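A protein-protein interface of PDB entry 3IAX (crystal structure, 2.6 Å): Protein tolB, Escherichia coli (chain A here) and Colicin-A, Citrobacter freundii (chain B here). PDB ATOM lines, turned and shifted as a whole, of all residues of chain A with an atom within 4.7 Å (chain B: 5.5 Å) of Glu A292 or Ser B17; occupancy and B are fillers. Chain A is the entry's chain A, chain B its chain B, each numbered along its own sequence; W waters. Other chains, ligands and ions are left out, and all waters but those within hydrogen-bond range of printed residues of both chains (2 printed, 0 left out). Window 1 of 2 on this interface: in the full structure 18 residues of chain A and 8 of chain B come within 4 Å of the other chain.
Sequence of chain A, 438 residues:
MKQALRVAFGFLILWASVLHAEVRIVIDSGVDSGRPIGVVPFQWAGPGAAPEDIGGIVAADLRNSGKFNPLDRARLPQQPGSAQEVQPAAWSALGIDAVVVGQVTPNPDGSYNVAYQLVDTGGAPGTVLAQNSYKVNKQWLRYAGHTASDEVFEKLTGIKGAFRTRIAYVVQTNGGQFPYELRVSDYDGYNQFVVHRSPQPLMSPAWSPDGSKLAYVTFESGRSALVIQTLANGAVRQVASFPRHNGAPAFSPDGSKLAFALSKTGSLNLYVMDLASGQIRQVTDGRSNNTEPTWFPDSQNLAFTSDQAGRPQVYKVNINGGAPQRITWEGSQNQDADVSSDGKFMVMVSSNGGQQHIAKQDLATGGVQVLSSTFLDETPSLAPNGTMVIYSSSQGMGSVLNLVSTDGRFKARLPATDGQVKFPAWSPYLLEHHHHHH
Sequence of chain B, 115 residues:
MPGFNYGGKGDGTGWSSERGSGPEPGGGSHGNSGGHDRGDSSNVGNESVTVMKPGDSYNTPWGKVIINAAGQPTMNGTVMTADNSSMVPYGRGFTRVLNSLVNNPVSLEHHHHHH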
ATOM      1  N   MET A 203      21.638  21.946 -27.304  1.00  0.00           N
ATOM      2  CA  MET A 203      21.943  20.564 -27.573  1.00  0.00           C
ATOM      3  C   MET A 203      20.832  19.843 -28.217  1.00  0.00           C
ATOM      4  O   MET A 203      19.702  20.211 -28.118  1.00  0.00           O
ATOM      5  CB  MET A 203      22.256  19.843 -26.304  1.00  0.00           C
ATOM      6  CG  MET A 203      23.157  20.546 -25.398  1.00  0.00           C
ATOM      7  SD  MET A 203      23.559  19.552 -24.036  1.00  0.00           S
ATOM      8  CE  MET A 203      25.208  19.576 -24.231  1.00  0.00           C
ATOM      9  N   SER A 204      21.226  18.777 -28.877  1.00  0.00           N
ATOM     10  CA  SER A 204      20.423  17.695 -29.354  1.00  0.00           C
ATOM     11  C   SER A 204      19.101  17.955 -30.007  1.00  0.00           C
ATOM     12  O   SER A 204      18.100  17.558 -29.503  1.00  0.00           O
ATOM     13  CB  SER A 204      20.115  16.794 -28.195  1.00  0.00           C
ATOM     14  OG  SER A 204      21.193  16.532 -27.411  1.00  0.00           O
ATOM     15  N   ALA A 248      17.778  15.543 -24.473  1.00  0.00           N
ATOM     16  CA  ALA A 248      17.671  14.466 -25.432  1.00  0.00           C
ATOM     17  C   ALA A 248      16.361  14.128 -26.039  1.00  0.00           C
ATOM     18  O   ALA A 248      15.903  13.062 -25.890  1.00  0.00           O
ATOM     19  CB  ALA A 248      18.277  13.281 -24.895  1.00  0.00           C
ATOM     20  N   THR A 291      19.472   7.714 -20.862  1.00  0.00           N
ATOM     21  CA  THR A 291      19.297   8.850 -21.740  1.00  0.00           C
ATOM     22  C   THR A 291      19.377   8.482 -23.215  1.00  0.00           C
ATOM     23  O   THR A 291      19.521   7.300 -23.554  1.00  0.00           O
ATOM     24  CB  THR A 291      20.267   9.978 -21.377  1.00  0.00           C
ATOM     25  OG1 THR A 291      19.886  11.162 -22.084  1.00  0.00           O
ATOM     26  CG2 THR A 291      21.726   9.599 -21.678  1.00  0.00           C
ATOM     27  N   GLU A 292      19.235   9.498 -24.074  1.00  0.00           N
ATOM     28  CA  GLU A 292      19.319   9.363 -25.538  1.00  0.00           C
ATOM     29  C   GLU A 292      18.285   8.393 -26.122  1.00  0.00           C
ATOM     30  O   GLU A 292      18.643   7.444 -26.817  1.00  0.00           O
ATOM     31  CB  GLU A 292      20.749   8.999 -25.985  1.00  0.00           C
ATOM     32  CG  GLU A 292      21.821   9.917 -25.400  1.00  0.00           C
ATOM     33  CD  GLU A 292      23.230   9.430 -25.670  1.00  0.00           C
ATOM     34  OE1 GLU A 292      23.538   8.243 -25.409  1.00  0.00           O
ATOM     35  OE2 GLU A 292      24.043  10.249 -26.140  1.00  0.00           O
ATOM     36  N   PRO A 293      16.996   8.625 -25.821  1.00  0.00           N
ATOM     37  CA  PRO A 293      15.916   7.834 -26.419  1.00  0.00           C
ATOM     38  C   PRO A 293      15.825   7.948 -27.937  1.00  0.00           C
ATOM     39  O   PRO A 293      16.126   8.997 -28.512  1.00  0.00           O
ATOM     40  CB  PRO A 293      14.651   8.448 -25.803  1.00  0.00           C
ATOM     41  CG  PRO A 293      15.070   9.818 -25.377  1.00  0.00           C
ATOM     42  CD  PRO A 293      16.468   9.636 -24.888  1.00  0.00           C
ATOM     43  N   THR A 294      15.430   6.854 -28.537  1.00  0.00           N
ATOM     44  CA  THR A 294      15.209   6.677 -29.938  1.00  0.00           C
ATOM     45  C   THR A 294      14.027   5.746 -30.149  1.00  0.00           C
ATOM     46  O   THR A 294      13.894   4.745 -29.556  1.00  0.00           O
ATOM     47  CB  THR A 294      16.495   6.284 -30.713  1.00  0.00           C
ATOM     48  OG1 THR A 294      16.370   6.624 -32.078  1.00  0.00           O
ATOM     49  CG2 THR A 294      16.832   4.918 -30.591  1.00  0.00           C
ATOM     50  N   ALA A 303      14.758   2.614 -27.755  1.00  0.00           N
ATOM     51  CA  ALA A 303      16.066   2.128 -27.496  1.00  0.00           C
ATOM     52  C   ALA A 303      16.700   3.336 -26.818  1.00  0.00           C
ATOM     53  O   ALA A 303      16.336   4.429 -27.063  1.00  0.00           O
ATOM     54  CB  ALA A 303      16.739   1.780 -28.740  1.00  0.00           C
ATOM     55  N   PHE A 304      17.618   3.120 -25.919  1.00  0.00           N
ATOM     56  CA  PHE A 304      18.284   4.219 -25.231  1.00  0.00           C
ATOM     57  C   PHE A 304      19.647   3.783 -24.715  1.00  0.00           C
ATOM     58  O   PHE A 304      20.042   2.624 -24.887  1.00  0.00           O
ATOM     59  CB  PHE A 304      17.397   4.760 -24.102  1.00  0.00           C
ATOM     60  CG  PHE A 304      17.070   3.745 -23.048  1.00  0.00           C
ATOM     61  CD1 PHE A 304      16.102   2.762 -23.276  1.00  0.00           C
ATOM     62  CD2 PHE A 304      17.723   3.764 -21.821  1.00  0.00           C
ATOM     63  CE1 PHE A 304      15.806   1.808 -22.293  1.00  0.00           C
ATOM     64  CE2 PHE A 304      17.422   2.821 -20.834  1.00  0.00           C
ATOM     65  CZ  PHE A 304      16.468   1.843 -21.070  1.00  0.00           C
ATOM     66  N   THR A 305      20.385   4.706 -24.101  1.00  0.00           N
ATOM     67  CA  THR A 305      21.677   4.361 -23.519  1.00  0.00           C
ATOM     68  C   THR A 305      21.601   4.352 -22.001  1.00  0.00           C
ATOM     69  O   THR A 305      20.986   5.232 -21.399  1.00  0.00           O
ATOM     70  CB  THR A 305      22.758   5.333 -23.953  1.00  0.00           C
ATOM     71  OG1 THR A 305      22.512   5.726 -25.308  1.00  0.00           O
ATOM     72  CG2 THR A 305      24.129   4.681 -23.843  1.00  0.00           C
ATOM     73  N   GLN A 335      26.664   3.549 -27.394  1.00  0.00           N
ATOM     74  CA  GLN A 335      25.785   4.588 -26.947  1.00  0.00           C
ATOM     75  C   GLN A 335      25.210   5.361 -28.109  1.00  0.00           C
ATOM     76  O   GLN A 335      25.645   5.194 -29.179  1.00  0.00           O
ATOM     77  CB  GLN A 335      26.597   5.523 -26.090  1.00  0.00           C
ATOM     78  CG  GLN A 335      27.945   5.687 -26.633  1.00  0.00           C
ATOM     79  CD  GLN A 335      28.847   6.474 -25.813  1.00  0.00           C
ATOM     80  OE1 GLN A 335      29.986   6.229 -25.809  1.00  0.00           O
ATOM     81  NE2 GLN A 335      28.361   7.450 -25.161  1.00  0.00           N
ATOM     82  N   ASP A 336      24.224   6.196 -27.855  1.00  0.00           N
ATOM     83  CA  ASP A 336      23.623   7.087 -28.840  1.00  0.00           C
ATOM     84  C   ASP A 336      22.978   6.437 -30.076  1.00  0.00           C
ATOM     85  O   ASP A 336      23.387   6.618 -31.180  1.00  0.00           O
ATOM     86  CB  ASP A 336      24.729   8.016 -29.235  1.00  0.00           C
ATOM     87  CG  ASP A 336      24.335   9.388 -29.239  1.00  0.00           C
ATOM     88  OD1 ASP A 336      23.171   9.674 -29.122  1.00  0.00           O
ATOM     89  OD2 ASP A 336      25.216  10.166 -29.412  1.00  0.00           O
ATOM     90  N   THR A 379      27.352  11.220 -32.257  1.00  0.00           N
ATOM     91  CA  THR A 379      26.004  11.508 -32.658  1.00  0.00           C
ATOM     92  C   THR A 379      25.482  11.080 -34.021  1.00  0.00           C
ATOM     93  O   THR A 379      25.139  11.913 -34.768  1.00  0.00           O
ATOM     94  CB  THR A 379      25.703  12.967 -32.368  1.00  0.00           C
ATOM     95  OG1 THR A 379      26.707  13.798 -32.914  1.00  0.00           O
ATOM     96  CG2 THR A 379      25.729  13.179 -30.959  1.00  0.00           C
ATOM     97  N   PHE A 423      25.934  17.737 -33.028  1.00  0.00           N
ATOM     98  CA  PHE A 423      24.583  17.286 -32.934  1.00  0.00           C
ATOM     99  C   PHE A 423      23.725  17.254 -34.167  1.00  0.00           C
ATOM    100  O   PHE A 423      22.674  17.793 -34.151  1.00  0.00           O
ATOM    101  CB  PHE A 423      23.856  18.131 -31.938  1.00  0.00           C
ATOM    102  CG  PHE A 423      24.260  17.944 -30.549  1.00  0.00           C
ATOM    103  CD1 PHE A 423      24.134  16.765 -29.926  1.00  0.00           C
ATOM    104  CD2 PHE A 423      24.748  18.989 -29.844  1.00  0.00           C
ATOM    105  CE1 PHE A 423      24.494  16.666 -28.633  1.00  0.00           C
ATOM    106  CE2 PHE A 423      25.107  18.856 -28.603  1.00  0.00           C
ATOM    107  CZ  PHE A 423      24.966  17.710 -27.994  1.00  0.00           C
ATOM    108  N   ASP B  11      24.882  17.249 -18.539  1.00  0.00           N
ATOM    109  CA  ASP B  11      23.966  16.329 -17.875  1.00  0.00           C
ATOM    110  C   ASP B  11      24.613  15.595 -16.697  1.00  0.00           C
ATOM    111  O   ASP B  11      23.934  14.877 -15.965  1.00  0.00           O
ATOM    112  CB  ASP B  11      23.278  15.372 -18.877  1.00  0.00           C
ATOM    113  CG  ASP B  11      24.195  14.262 -19.392  1.00  0.00           C
ATOM    114  OD1 ASP B  11      25.389  14.195 -19.009  1.00  0.00           O
ATOM    115  OD2 ASP B  11      23.709  13.439 -20.197  1.00  0.00           O
ATOM    116  N   TRP B  15      29.801  10.512 -19.813  1.00  0.00           N
ATOM    117  CA  TRP B  15      29.833   9.683 -20.979  1.00  0.00           C
ATOM    118  C   TRP B  15      29.003  10.101 -22.167  1.00  0.00           C
ATOM    119  O   TRP B  15      29.385   9.811 -23.259  1.00  0.00           O
ATOM    120  CB  TRP B  15      29.511   8.246 -20.634  1.00  0.00           C
ATOM    121  CG  TRP B  15      28.321   8.008 -19.900  1.00  0.00           C
ATOM    122  CD1 TRP B  15      28.218   7.904 -18.592  1.00  0.00           C
ATOM    123  CD2 TRP B  15      27.041   7.788 -20.422  1.00  0.00           C
ATOM    124  NE1 TRP B  15      26.956   7.657 -18.234  1.00  0.00           N
ATOM    125  CE2 TRP B  15      26.203   7.577 -19.361  1.00  0.00           C
ATOM    126  CE3 TRP B  15      26.513   7.758 -21.690  1.00  0.00           C
ATOM    127  CZ2 TRP B  15      24.889   7.314 -19.526  1.00  0.00           C
ATOM    128  CZ3 TRP B  15      25.238   7.513 -21.836  1.00  0.00           C
ATOM    129  CH2 TRP B  15      24.435   7.265 -20.773  1.00  0.00           C
ATOM    130  N   SER B  16      27.841  10.697 -21.911  1.00  0.00           N
ATOM    131  CA  SER B  16      26.849  11.030 -22.940  1.00  0.00           C
ATOM    132  C   SER B  16      27.156  12.121 -23.965  1.00  0.00           C
ATOM    133  O   SER B  16      28.192  12.786 -23.915  1.00  0.00           O
ATOM    134  CB  SER B  16      25.498  11.329 -22.279  1.00  0.00           C
ATOM    135  OG  SER B  16      25.599  12.423 -21.384  1.00  0.00           O
ATOM    136  N   SER B  17      26.215  12.282 -24.895  1.00  0.00           N
ATOM    137  CA  SER B  17      26.295  13.248 -25.935  1.00  0.00           C
ATOM    138  C   SER B  17      26.129  14.583 -25.366  1.00  0.00           C
ATOM    139  O   SER B  17      26.469  15.549 -25.989  1.00  0.00           O
ATOM    140  CB  SER B  17      25.231  12.989 -26.980  1.00  0.00           C
ATOM    141  OG  SER B  17      23.962  13.035 -26.444  1.00  0.00           O
ATOM    142  N   GLU B  18      25.644  14.618 -24.142  1.00  0.00           N
ATOM    143  CA  GLU B  18      25.243  15.828 -23.500  1.00  0.00           C
ATOM    144  C   GLU B  18      25.920  16.149 -22.196  1.00  0.00           C
ATOM    145  O   GLU B  18      25.287  16.630 -21.321  1.00  0.00           O
ATOM    146  CB  GLU B  18      23.762  15.735 -23.241  1.00  0.00           C
ATOM    147  CG  GLU B  18      22.943  15.859 -24.430  1.00  0.00           C
ATOM    148  CD  GLU B  18      21.505  15.887 -24.139  1.00  0.00           C
ATOM    149  OE1 GLU B  18      21.096  15.518 -23.085  1.00  0.00           O
ATOM    150  OE2 GLU B  18      20.754  16.259 -24.989  1.00  0.00           O
ATOM    151  N   ARG B  19      27.208  15.907 -22.071  1.00  0.00           N
ATOM    152  CA  ARG B  19      27.957  16.114 -20.817  1.00  0.00           C
ATOM    153  C   ARG B  19      28.449  17.529 -20.630  1.00  0.00           C
ATOM    154  O   ARG B  19      28.399  18.052 -19.522  1.00  0.00           O
ATOM    155  CB  ARG B  19      29.205  15.240 -20.732  1.00  0.00           C
ATOM    156  CG  ARG B  19      29.317  14.131 -21.708  1.00  0.00           C
ATOM    157  CD  ARG B  19      30.783  13.923 -22.036  1.00  0.00           C
ATOM    158  NE  ARG B  19      31.074  14.288 -23.416  1.00  0.00           N
ATOM    159  CZ  ARG B  19      31.713  13.505 -24.280  1.00  0.00           C
ATOM    160  NH1 ARG B  19      32.161  12.310 -23.895  1.00  0.00           N
ATOM    161  NH2 ARG B  19      31.924  13.925 -25.521  1.00  0.00           N
HETATM  162  O   HOH W   1      21.285  13.388 -21.058  1.00  0.00           O
HETATM  163  O   HOH W   2      21.756  13.559 -28.005  1.00  0.00           O
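OE2 of Glu A292 is in hydrogen-bond range of OG of Ser B17 (2.8 Å). N of Ala A248 sits at hydrogen-bond distance from OE2 of Glu B18, 3.1 Å away. The side-chain amide nitrogen (NE2) of Gln A335 is in hydrogen-bond range of the backbone carbonyl oxygen (O) of Trp B15, 3.2 Å away. The side-chain hydroxyl (OG) of Ser A204 lies within hydrogen-bond range of the side-chain carboxylate (OE2) of Glu B18 (2.5 Å).
The backbone carbonyl oxygen (O) of Thr A291 lies within hydrogen-bond range of the backbone NH (N) of Thr A305 (2.8 Å). N of Asp A336 sits at hydrogen-bond distance from OG1 of Thr A305 (3.1 Å). N of Asp B11 is in hydrogen-bond range of O of Glu B18. The backbone NH (N) of Asp A336 lies within hydrogen-bond range of the side-chain carboxylate (OE1) of Glu A292. OG1 of Thr A305 is in hydrogen-bond range of OE1 of Glu A292.
Met A203 touches Glu B18. CG2 of Thr A291 touches CH2 of Trp B15 (3.7 Å). Trp B15 touches Thr A305. Asp A336 touches Ser B17 (OD2 to CB, 3.7 Å). O of Ser B17 touches CZ of Phe A423 (3.3 Å).
Printed residues of chain B within 4 Å of Met A203: Glu B18 (3.8 Å). Printed residues of chain B within 4 Å of Ser A204: Glu B18 (2.5 Å). Of chain B, only Ser B17 (2.8 Å) comes within 4 Å of Glu A292. Of the printed residues of chain B, Asp A336 touches Ser B17. Printed residues of chain B within 4 Å of Phe A423: Ser B17. Of the printed residues of chain A, Glu B18 touches Met A203, Ser A204 and Ala A248. The nearest printed residue of chain B that does not touch Met A203 is Ser B17 (4.6 Å).
Hydrophobic or aromatic side chains of chain A within 4 Å of the printed part of chain B: Met A203, Ala A248 and Phe A423. Of the 6 printed residues of chain B, 3 touch a printed residue of chain A. Hydrophobic or aromatic side chains of chain B that line the printed part of chain A: Trp B15. Among the printed residues, no Asp or Glu carboxylate lies within 4 Å of a Lys or Arg side-chain nitrogen of the other chain.
Water W1 lies within hydrogen-bond range of the side-chain carboxylate (OD2) of Asp B11, the side-chain hydroxyl (OG1) of Thr A291 and the side-chain carboxylate (OE1) of Glu B18. Water W2 bridges OG of Ser B17 and OG of Ser A204.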
